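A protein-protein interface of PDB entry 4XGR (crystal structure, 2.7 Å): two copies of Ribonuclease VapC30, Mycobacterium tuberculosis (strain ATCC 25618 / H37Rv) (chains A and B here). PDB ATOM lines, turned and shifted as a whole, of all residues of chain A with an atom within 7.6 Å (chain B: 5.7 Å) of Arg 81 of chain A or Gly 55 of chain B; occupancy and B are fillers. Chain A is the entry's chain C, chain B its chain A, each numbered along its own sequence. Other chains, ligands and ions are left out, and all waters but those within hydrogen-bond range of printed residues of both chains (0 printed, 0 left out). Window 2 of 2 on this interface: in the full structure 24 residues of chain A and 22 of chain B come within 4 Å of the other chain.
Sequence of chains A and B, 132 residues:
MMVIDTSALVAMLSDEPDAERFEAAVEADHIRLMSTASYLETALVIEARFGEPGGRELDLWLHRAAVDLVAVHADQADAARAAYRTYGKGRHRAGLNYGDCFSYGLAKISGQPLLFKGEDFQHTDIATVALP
The side-chain hydroxyl of Tyr 39 of chain B is in hydrogen-bond range of the guanidinium group of Arg 81 of chain A, 2.7 Å away. OD1 of Asp 78 of chain A is in hydrogen-bond range of OH of Tyr 39 of chain B (2.7 Å). OE2 of Glu 47 of chain B lies within salt-bridge range of NH2 of Arg 85 of chain A. The guanidinium group of Arg 81 of chain A is in salt-bridge range of the side-chain carboxylate of Glu 47 of chain B. NH1 of Arg 85 of chain A is in salt-bridge range of OE1 of Glu 52 of chain B (3.5 Å). The guanidinium group (NH1) of Arg 81 of chain A is in salt-bridge range of the side-chain carboxylate (OD1) of Asp 59 of chain B, 2.5 Å away. O of Gly 55 of chain B is in hydrogen-bond range of NH2 of Arg 81 of chain A (3.1 Å).
Hydrophobic or aromatic side chains of chain B within 4 Å of the printed part of chain A: Tyr 39, Leu 40, Ala 43 and Leu 44. Of the 16 printed residues of chain A, 7 touch a printed residue of chain B.
Ala 74 of chain A touches none of the printed residues of chain B. Of the printed residues of chain B, Ala 77 of chain A touches Tyr 39 (3.9 Å) and Leu 40 (3.4 Å). Arg 81 of chain A touches just these residues of chain B: Tyr 39 (2.7 Å), Leu 40 (3.6 Å), Ala 43 (3.6 Å), Glu 47 (2.8 Å), Gly 55 (3.1 Å) and Asp 59 (2.5 Å). Printed residues of chain B within 4 Å of Arg 85 of chain A: Glu 47 (2.7 Å) and Glu 52 (3.5 Å). Of the printed residues of chain B, Cys 101 of chain A touches Leu 40 (3.8 Å). Printed residues of chain A within 4 Å of Leu 40 of chain B: Ala 77, Ala 80, Arg 81 and Cys 101. Printed residues of chain A within 4 Å of Ala 43 of chain B: Arg 81 (3.6 Å). Gly 55 of chain B touches just one residue of chain A: Arg 81 (3.1 Å). Glu 57 of chain B touches none of the printed residues of chain A. The nearest printed residue of chain B that does not touch Ala 77 of chain A is Ala 43 of chain B (6.4 Å).
Tyr 39 of chain B touches Ala 77 of chain A. O of Ala 77 of chain A touches CD1 of Leu 40 of chain B, 3.4 Å away. CB of Ala 80 of chain A touches CD1 of Leu 40 of chain B, at 3.96 Å. Leu 40 of chain B touches Arg 81 of chain A. Arg 81 of chain A touches Ala 43 of chain B. CG of Tyr 84 of chain A touches CD2 of Leu 44 of chain B, at 3.4 Å. CD2 of Leu 40 of chain B touches CB of Cys 101 of chain A (3.8 Å).
No position is printed for both chains.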
ATOM      1  N   ALA A  74      25.170  -4.883  30.985  1.00  0.00           N
ATOM      2  CA  ALA A  74      24.249  -4.155  30.110  1.00  0.00           C
ATOM      3  C   ALA A  74      22.808  -4.232  30.617  1.00  0.00           C
ATOM      4  O   ALA A  74      22.018  -3.255  30.518  1.00  0.00           O
ATOM      5  CB  ALA A  74      24.348  -4.701  28.686  1.00  0.00           C
ATOM      6  N   ASP A  75      22.456  -5.398  31.152  1.00  0.00           N
ATOM      7  CA  ASP A  75      21.074  -5.623  31.584  1.00  0.00           C
ATOM      8  C   ASP A  75      20.684  -4.669  32.709  1.00  0.00           C
ATOM      9  O   ASP A  75      19.532  -4.210  32.752  1.00  0.00           O
ATOM     10  CB  ASP A  75      20.785  -7.108  31.910  1.00  0.00           C
ATOM     11  CG  ASP A  75      21.700  -7.702  32.985  1.00  0.00           C
ATOM     12  OD1 ASP A  75      22.445  -6.962  33.657  1.00  0.00           O
ATOM     13  OD2 ASP A  75      21.666  -8.934  33.155  1.00  0.00           O
ATOM     14  N   GLN A  76      21.653  -4.337  33.575  1.00  0.00           N
ATOM     15  CA  GLN A  76      21.440  -3.368  34.662  1.00  0.00           C
ATOM     16  C   GLN A  76      21.257  -1.973  34.111  1.00  0.00           C
ATOM     17  O   GLN A  76      20.341  -1.238  34.520  1.00  0.00           O
ATOM     18  CB  GLN A  76      22.620  -3.359  35.634  1.00  0.00           C
ATOM     19  CG  GLN A  76      22.838  -4.688  36.336  1.00  0.00           C
ATOM     20  CD  GLN A  76      24.149  -4.734  37.044  1.00  0.00           C
ATOM     21  OE1 GLN A  76      24.620  -3.723  37.521  1.00  0.00           O
ATOM     22  NE2 GLN A  76      24.748  -5.904  37.117  1.00  0.00           N
ATOM     23  N   ALA A  77      22.131  -1.605  33.179  1.00  0.00           N
ATOM     24  CA  ALA A  77      22.034  -0.313  32.513  1.00  0.00           C
ATOM     25  C   ALA A  77      20.688  -0.099  31.798  1.00  0.00           C
ATOM     26  O   ALA A  77      20.220   1.031  31.751  1.00  0.00           O
ATOM     27  CB  ALA A  77      23.191  -0.137  31.553  1.00  0.00           C
ATOM     28  N   ASP A  78      20.063  -1.169  31.277  1.00  0.00           N
ATOM     29  CA  ASP A  78      18.734  -1.090  30.602  1.00  0.00           C
ATOM     30  C   ASP A  78      17.564  -0.930  31.573  1.00  0.00           C
ATOM     31  O   ASP A  78      16.531  -0.340  31.220  1.00  0.00           O
ATOM     32  CB  ASP A  78      18.468  -2.340  29.729  1.00  0.00           C
ATOM     33  CG  ASP A  78      19.425  -2.447  28.517  1.00  0.00           C
ATOM     34  OD1 ASP A  78      19.963  -1.394  28.041  1.00  0.00           O
ATOM     35  OD2 ASP A  78      19.632  -3.603  28.044  1.00  0.00           O
ATOM     36  N   ALA A  79      17.679  -1.487  32.773  1.00  0.00           N
ATOM     37  CA  ALA A  79      16.623  -1.306  33.787  1.00  0.00           C
ATOM     38  C   ALA A  79      16.610   0.115  34.325  1.00  0.00           C
ATOM     39  O   ALA A  79      15.558   0.655  34.679  1.00  0.00           O
ATOM     40  CB  ALA A  79      16.801  -2.291  34.921  1.00  0.00           C
ATOM     41  N   ALA A  80      17.788   0.725  34.366  1.00  0.00           N
ATOM     42  CA  ALA A  80      17.937   2.060  34.889  1.00  0.00           C
ATOM     43  C   ALA A  80      17.415   3.011  33.861  1.00  0.00           C
ATOM     44  O   ALA A  80      16.565   3.845  34.170  1.00  0.00           O
ATOM     45  CB  ALA A  80      19.394   2.354  35.207  1.00  0.00           C
ATOM     46  N   ARG A  81      17.944   2.906  32.643  1.00  0.00           N
ATOM     47  CA  ARG A  81      17.430   3.672  31.510  1.00  0.00           C
ATOM     48  C   ARG A  81      15.896   3.612  31.511  1.00  0.00           C
ATOM     49  O   ARG A  81      15.241   4.639  31.661  1.00  0.00           O
ATOM     50  CB  ARG A  81      17.991   3.107  30.206  1.00  0.00           C
ATOM     51  CG  ARG A  81      17.499   3.805  28.955  1.00  0.00           C
ATOM     52  CD  ARG A  81      18.025   3.093  27.719  1.00  0.00           C
ATOM     53  NE  ARG A  81      17.358   3.565  26.510  1.00  0.00           N
ATOM     54  CZ  ARG A  81      17.696   3.223  25.262  1.00  0.00           C
ATOM     55  NH1 ARG A  81      18.704   2.368  25.016  1.00  0.00           N
ATOM     56  NH2 ARG A  81      16.996   3.735  24.251  1.00  0.00           N
ATOM     57  N   ALA A  82      15.363   2.394  31.427  1.00  0.00           N
ATOM     58  CA  ALA A  82      13.930   2.127  31.509  1.00  0.00           C
ATOM     59  C   ALA A  82      13.238   2.844  32.663  1.00  0.00           C
ATOM     60  O   ALA A  82      12.255   3.551  32.449  1.00  0.00           O
ATOM     61  CB  ALA A  82      13.667   0.617  31.602  1.00  0.00           C
ATOM     62  N   ALA A  83      13.758   2.662  33.876  1.00  0.00           N
ATOM     63  CA  ALA A  83      13.120   3.191  35.083  1.00  0.00           C
ATOM     64  C   ALA A  83      13.259   4.690  35.295  1.00  0.00           C
ATOM     65  O   ALA A  83      12.572   5.242  36.138  1.00  0.00           O
ATOM     66  CB  ALA A  83      13.661   2.469  36.306  1.00  0.00           C
ATOM     67  N   TYR A  84      14.167   5.343  34.577  1.00  0.00           N
ATOM     68  CA  TYR A  84      14.476   6.763  34.818  1.00  0.00           C
ATOM     69  C   TYR A  84      13.385   7.699  34.335  1.00  0.00           C
ATOM     70  O   TYR A  84      13.211   8.774  34.896  1.00  0.00           O
ATOM     71  CB  TYR A  84      15.775   7.155  34.120  1.00  0.00           C
ATOM     72  CG  TYR A  84      16.390   8.438  34.605  1.00  0.00           C
ATOM     73  CD1 TYR A  84      17.227   8.435  35.707  1.00  0.00           C
ATOM     74  CD2 TYR A  84      16.183   9.641  33.941  1.00  0.00           C
ATOM     75  CE1 TYR A  84      17.825   9.593  36.158  1.00  0.00           C
ATOM     76  CE2 TYR A  84      16.780  10.819  34.394  1.00  0.00           C
ATOM     77  CZ  TYR A  84      17.600  10.778  35.512  1.00  0.00           C
ATOM     78  OH  TYR A  84      18.227  11.898  35.997  1.00  0.00           O
ATOM     79  N   ARG A  85      12.654   7.288  33.303  1.00  0.00           N
ATOM     80  CA  ARG A  85      11.606   8.129  32.718  1.00  0.00           C
ATOM     81  C   ARG A  85      10.449   8.299  33.700  1.00  0.00           C
ATOM     82  O   ARG A  85       9.749   9.305  33.676  1.00  0.00           O
ATOM     83  CB  ARG A  85      11.079   7.533  31.404  1.00  0.00           C
ATOM     84  CG  ARG A  85      12.141   7.166  30.360  1.00  0.00           C
ATOM     85  CD  ARG A  85      11.780   5.827  29.753  1.00  0.00           C
ATOM     86  NE  ARG A  85      12.865   5.159  29.062  1.00  0.00           N
ATOM     87  CZ  ARG A  85      12.764   3.941  28.530  1.00  0.00           C
ATOM     88  NH1 ARG A  85      11.628   3.258  28.615  1.00  0.00           N
ATOM     89  NH2 ARG A  85      13.803   3.391  27.919  1.00  0.00           N
ATOM     90  N   THR A  86      10.273   7.305  34.565  1.00  0.00           N
ATOM     91  CA  THR A  86       9.255   7.333  35.595  1.00  0.00           C
ATOM     92  C   THR A  86       9.756   7.934  36.900  1.00  0.00           C
ATOM     93  O   THR A  86       9.086   8.788  37.467  1.00  0.00           O
ATOM     94  CB  THR A  86       8.747   5.918  35.849  1.00  0.00           C
ATOM     95  OG1 THR A  86       9.859   5.066  36.129  1.00  0.00           O
ATOM     96  CG2 THR A  86       8.036   5.392  34.619  1.00  0.00           C
ATOM     97  N   CYS A 101      21.311   5.426  39.531  1.00  0.00           N
ATOM     98  CA  CYS A 101      20.958   4.433  38.506  1.00  0.00           C
ATOM     99  C   CYS A 101      21.666   3.080  38.658  1.00  0.00           C
ATOM    100  O   CYS A 101      21.055   2.034  38.404  1.00  0.00           O
ATOM    101  CB  CYS A 101      21.161   4.994  37.098  1.00  0.00           C
ATOM    102  SG  CYS A 101      19.850   6.134  36.596  1.00  0.00           S
ATOM    103  N   TYR A 104      20.080   1.243  41.639  1.00  0.00           N
ATOM    104  CA  TYR A 104      18.809   0.766  41.098  1.00  0.00           C
ATOM    105  C   TYR A 104      19.029  -0.412  40.166  1.00  0.00           C
ATOM    106  O   TYR A 104      18.329  -1.420  40.283  1.00  0.00           O
ATOM    107  CB  TYR A 104      18.057   1.859  40.339  1.00  0.00           C
ATOM    108  CG  TYR A 104      16.691   1.419  39.843  1.00  0.00           C
ATOM    109  CD1 TYR A 104      16.544   0.717  38.634  1.00  0.00           C
ATOM    110  CD2 TYR A 104      15.534   1.705  40.577  1.00  0.00           C
ATOM    111  CE1 TYR A 104      15.295   0.308  38.187  1.00  0.00           C
ATOM    112  CE2 TYR A 104      14.281   1.310  40.124  1.00  0.00           C
ATOM    113  CZ  TYR A 104      14.168   0.612  38.934  1.00  0.00           C
ATOM    114  OH  TYR A 104      12.926   0.216  38.494  1.00  0.00           O
ATOM    115  N   GLY A 105      19.982  -0.275  39.244  1.00  0.00           N
ATOM    116  CA  GLY A 105      20.210  -1.283  38.222  1.00  0.00           C
ATOM    117  C   GLY A 105      20.466  -2.645  38.826  1.00  0.00           C
ATOM    118  O   GLY A 105      19.679  -3.583  38.631  1.00  0.00           O
ATOM    119  N   TYR B  39      27.101   4.603  27.838  1.00  0.00           N
ATOM    120  CA  TYR B  39      25.837   4.256  27.131  1.00  0.00           C
ATOM    121  C   TYR B  39      24.581   4.676  27.899  1.00  0.00           C
ATOM    122  O   TYR B  39      23.641   5.243  27.321  1.00  0.00           O
ATOM    123  CB  TYR B  39      25.722   2.749  26.890  1.00  0.00           C
ATOM    124  CG  TYR B  39      24.293   2.251  26.868  1.00  0.00           C
ATOM    125  CD1 TYR B  39      23.428   2.594  25.799  1.00  0.00           C
ATOM    126  CD2 TYR B  39      23.775   1.460  27.918  1.00  0.00           C
ATOM    127  CE1 TYR B  39      22.115   2.170  25.769  1.00  0.00           C
ATOM    128  CE2 TYR B  39      22.451   1.014  27.885  1.00  0.00           C
ATOM    129  CZ  TYR B  39      21.624   1.384  26.812  1.00  0.00           C
ATOM    130  OH  TYR B  39      20.309   0.977  26.737  1.00  0.00           O
ATOM    131  N   LEU B  40      24.545   4.312  29.179  1.00  0.00           N
ATOM    132  CA  LEU B  40      23.471   4.698  30.085  1.00  0.00           C
ATOM    133  C   LEU B  40      23.349   6.205  30.160  1.00  0.00           C
ATOM    134  O   LEU B  40      22.245   6.710  30.156  1.00  0.00           O
ATOM    135  CB  LEU B  40      23.700   4.116  31.491  1.00  0.00           C
ATOM    136  CG  LEU B  40      22.744   4.555  32.612  1.00  0.00           C
ATOM    137  CD1 LEU B  40      21.310   4.163  32.256  1.00  0.00           C
ATOM    138  CD2 LEU B  40      23.151   3.994  33.976  1.00  0.00           C
ATOM    139  N   ALA B  43      21.804   7.696  26.989  1.00  0.00           N
ATOM    140  CA  ALA B  43      20.401   7.294  26.996  1.00  0.00           C
ATOM    141  C   ALA B  43      19.550   8.284  27.741  1.00  0.00           C
ATOM    142  O   ALA B  43      18.574   8.747  27.206  1.00  0.00           O
ATOM    143  CB  ALA B  43      20.213   5.910  27.573  1.00  0.00           C
ATOM    144  N   LEU B  44      19.943   8.634  28.957  1.00  0.00           N
ATOM    145  CA  LEU B  44      19.149   9.540  29.794  1.00  0.00           C
ATOM    146  C   LEU B  44      19.064  10.936  29.180  1.00  0.00           C
ATOM    147  O   LEU B  44      18.005  11.562  29.224  1.00  0.00           O
ATOM    148  CB  LEU B  44      19.756   9.652  31.196  1.00  0.00           C
ATOM    149  CG  LEU B  44      19.857   8.373  32.041  1.00  0.00           C
ATOM    150  CD1 LEU B  44      20.380   8.707  33.428  1.00  0.00           C
ATOM    151  CD2 LEU B  44      18.528   7.644  32.116  1.00  0.00           C
ATOM    152  N   ILE B  46      19.547  11.746  25.911  1.00  0.00           N
ATOM    153  CA  ILE B  46      18.810  11.658  24.643  1.00  0.00           C
ATOM    154  C   ILE B  46      17.320  11.486  24.939  1.00  0.00           C
ATOM    155  O   ILE B  46      16.507  12.285  24.476  1.00  0.00           O
ATOM    156  CB  ILE B  46      19.298  10.481  23.749  1.00  0.00           C
ATOM    157  CG1 ILE B  46      20.764  10.647  23.333  1.00  0.00           C
ATOM    158  CG2 ILE B  46      18.419  10.319  22.509  1.00  0.00           C
ATOM    159  CD1 ILE B  46      21.056  11.880  22.519  1.00  0.00           C
ATOM    160  N   GLU B  47      16.973  10.452  25.711  1.00  0.00           N
ATOM    161  CA  GLU B  47      15.565  10.120  25.974  1.00  0.00           C
ATOM    162  C   GLU B  47      14.838  11.248  26.650  1.00  0.00           C
ATOM    163  O   GLU B  47      13.669  11.468  26.378  1.00  0.00           O
ATOM    164  CB  GLU B  47      15.409   8.875  26.844  1.00  0.00           C
ATOM    165  CG  GLU B  47      15.593   7.560  26.113  1.00  0.00           C
ATOM    166  CD  GLU B  47      15.340   6.363  27.013  1.00  0.00           C
ATOM    167  OE1 GLU B  47      15.392   6.514  28.254  1.00  0.00           O
ATOM    168  OE2 GLU B  47      15.114   5.254  26.497  1.00  0.00           O
ATOM    169  N   GLY B  51      12.456  12.294  23.880  1.00  0.00           N
ATOM    170  CA  GLY B  51      11.582  11.159  24.183  1.00  0.00           C
ATOM    171  C   GLY B  51      12.201   9.824  23.780  1.00  0.00           C
ATOM    172  O   GLY B  51      13.326   9.764  23.282  1.00  0.00           O
ATOM    173  N   GLU B  52      11.441   8.753  23.970  1.00  0.00           N
ATOM    174  CA  GLU B  52      11.852   7.412  23.572  1.00  0.00           C
ATOM    175  C   GLU B  52      12.046   7.206  22.065  1.00  0.00           C
ATOM    176  O   GLU B  52      12.724   6.241  21.661  1.00  0.00           O
ATOM    177  CB  GLU B  52      10.850   6.381  24.088  1.00  0.00           C
ATOM    178  CG  GLU B  52      10.747   6.313  25.606  1.00  0.00           C
ATOM    179  CD  GLU B  52       9.763   5.257  26.045  1.00  0.00           C
ATOM    180  OE1 GLU B  52       9.977   4.078  25.673  1.00  0.00           O
ATOM    181  OE2 GLU B  52       8.767   5.592  26.735  1.00  0.00           O
ATOM    182  N   PRO B  53      11.440   8.067  21.219  1.00  0.00           N
ATOM    183  CA  PRO B  53      11.878   8.019  19.812  1.00  0.00           C
ATOM    184  C   PRO B  53      13.348   8.417  19.634  1.00  0.00           C
ATOM    185  O   PRO B  53      13.992   7.965  18.692  1.00  0.00           O
ATOM    186  CB  PRO B  53      10.936   8.998  19.106  1.00  0.00           C
ATOM    187  CG  PRO B  53       9.720   9.017  19.958  1.00  0.00           C
ATOM    188  CD  PRO B  53      10.217   8.875  21.374  1.00  0.00           C
ATOM    189  N   GLY B  54      13.866   9.247  20.531  1.00  0.00           N
ATOM    190  CA  GLY B  54      15.300   9.496  20.605  1.00  0.00           C
ATOM    191  C   GLY B  54      16.046   8.232  21.002  1.00  0.00           C
ATOM    192  O   GLY B  54      17.019   7.831  20.332  1.00  0.00           O
ATOM    193  N   GLY B  55      15.571   7.600  22.081  1.00  0.00           N
ATOM    194  CA  GLY B  55      16.106   6.318  22.533  1.00  0.00           C
ATOM    195  C   GLY B  55      16.177   5.307  21.418  1.00  0.00           C
ATOM    196  O   GLY B  55      17.175   4.612  21.251  1.00  0.00           O
ATOM    197  N   ARG B  56      15.109   5.249  20.635  1.00  0.00           N
ATOM    198  CA  ARG B  56      15.045   4.378  19.459  1.00  0.00           C
ATOM    199  C   ARG B  56      16.193   4.686  18.513  1.00  0.00           C
ATOM    200  O   ARG B  56      16.914   3.773  18.098  1.00  0.00           O
ATOM    201  CB  ARG B  56      13.686   4.554  18.755  1.00  0.00           C
ATOM    202  CG  ARG B  56      13.506   3.784  17.457  1.00  0.00           C
ATOM    203  CD  ARG B  56      13.698   2.297  17.655  1.00  0.00           C
ATOM    204  NE  ARG B  56      13.581   1.564  16.400  1.00  0.00           N
ATOM    205  CZ  ARG B  56      13.908   0.278  16.237  1.00  0.00           C
ATOM    206  NH1 ARG B  56      14.377  -0.449  17.258  1.00  0.00           N
ATOM    207  NH2 ARG B  56      13.770  -0.289  15.035  1.00  0.00           N
ATOM    208  N   GLU B  57      16.389   5.973  18.197  1.00  0.00           N
ATOM    209  CA  GLU B  57      17.517   6.372  17.332  1.00  0.00           C
ATOM    210  C   GLU B  57      18.885   6.076  17.956  1.00  0.00           C
ATOM    211  O   GLU B  57      19.842   5.798  17.235  1.00  0.00           O
ATOM    212  CB  GLU B  57      17.428   7.852  16.899  1.00  0.00           C
ATOM    213  CG  GLU B  57      16.200   8.253  16.070  1.00  0.00           C
ATOM    214  CD  GLU B  57      15.915   7.340  14.890  1.00  0.00           C
ATOM    215  OE1 GLU B  57      16.855   7.019  14.139  1.00  0.00           O
ATOM    216  OE2 GLU B  57      14.741   6.946  14.707  1.00  0.00           O
ATOM    217  N   LEU B  58      18.989   6.141  19.280  1.00  0.00           N
ATOM    218  CA  LEU B  58      20.223   5.732  19.974  1.00  0.00           C
ATOM    219  C   LEU B  58      20.476   4.267  19.735  1.00  0.00           C
ATOM    220  O   LEU B  58      21.541   3.891  19.257  1.00  0.00           O
ATOM    221  CB  LEU B  58      20.159   6.001  21.485  1.00  0.00           C
ATOM    222  CG  LEU B  58      21.294   5.453  22.378  1.00  0.00           C
ATOM    223  CD1 LEU B  58      22.661   5.695  21.767  1.00  0.00           C
ATOM    224  CD2 LEU B  58      21.237   6.058  23.779  1.00  0.00           C
ATOM    225  N   ASP B  59      19.487   3.441  20.056  1.00  0.00           N
ATOM    226  CA  ASP B  59      19.629   1.992  19.907  1.00  0.00           C
ATOM    227  C   ASP B  59      19.978   1.576  18.477  1.00  0.00           C
ATOM    228  O   ASP B  59      20.704   0.618  18.278  1.00  0.00           O
ATOM    229  CB  ASP B  59      18.362   1.293  20.398  1.00  0.00           C
ATOM    230  CG  ASP B  59      18.047   1.625  21.848  1.00  0.00           C
ATOM    231  OD1 ASP B  59      19.002   1.746  22.648  1.00  0.00           O
ATOM    232  OD2 ASP B  59      16.858   1.809  22.213  1.00  0.00           O
ATOM    233  N   LEU B  60      19.467   2.317  17.491  1.00  0.00           N
ATOM    234  CA  LEU B  60      19.729   2.052  16.065  1.00  0.00           C
ATOM    235  C   LEU B  60      21.132   2.458  15.633  1.00  0.00           C
ATOM    236  O   LEU B  60      21.765   1.767  14.823  1.00  0.00           O
ATOM    237  CB  LEU B  60      18.683   2.759  15.195  1.00  0.00           C
ATOM    238  CG  LEU B  60      17.288   2.108  15.269  1.00  0.00           C
ATOM    239  CD1 LEU B  60      16.215   3.095  14.832  1.00  0.00           C
ATOM    240  CD2 LEU B  60      17.220   0.837  14.426  1.00  0.00           C
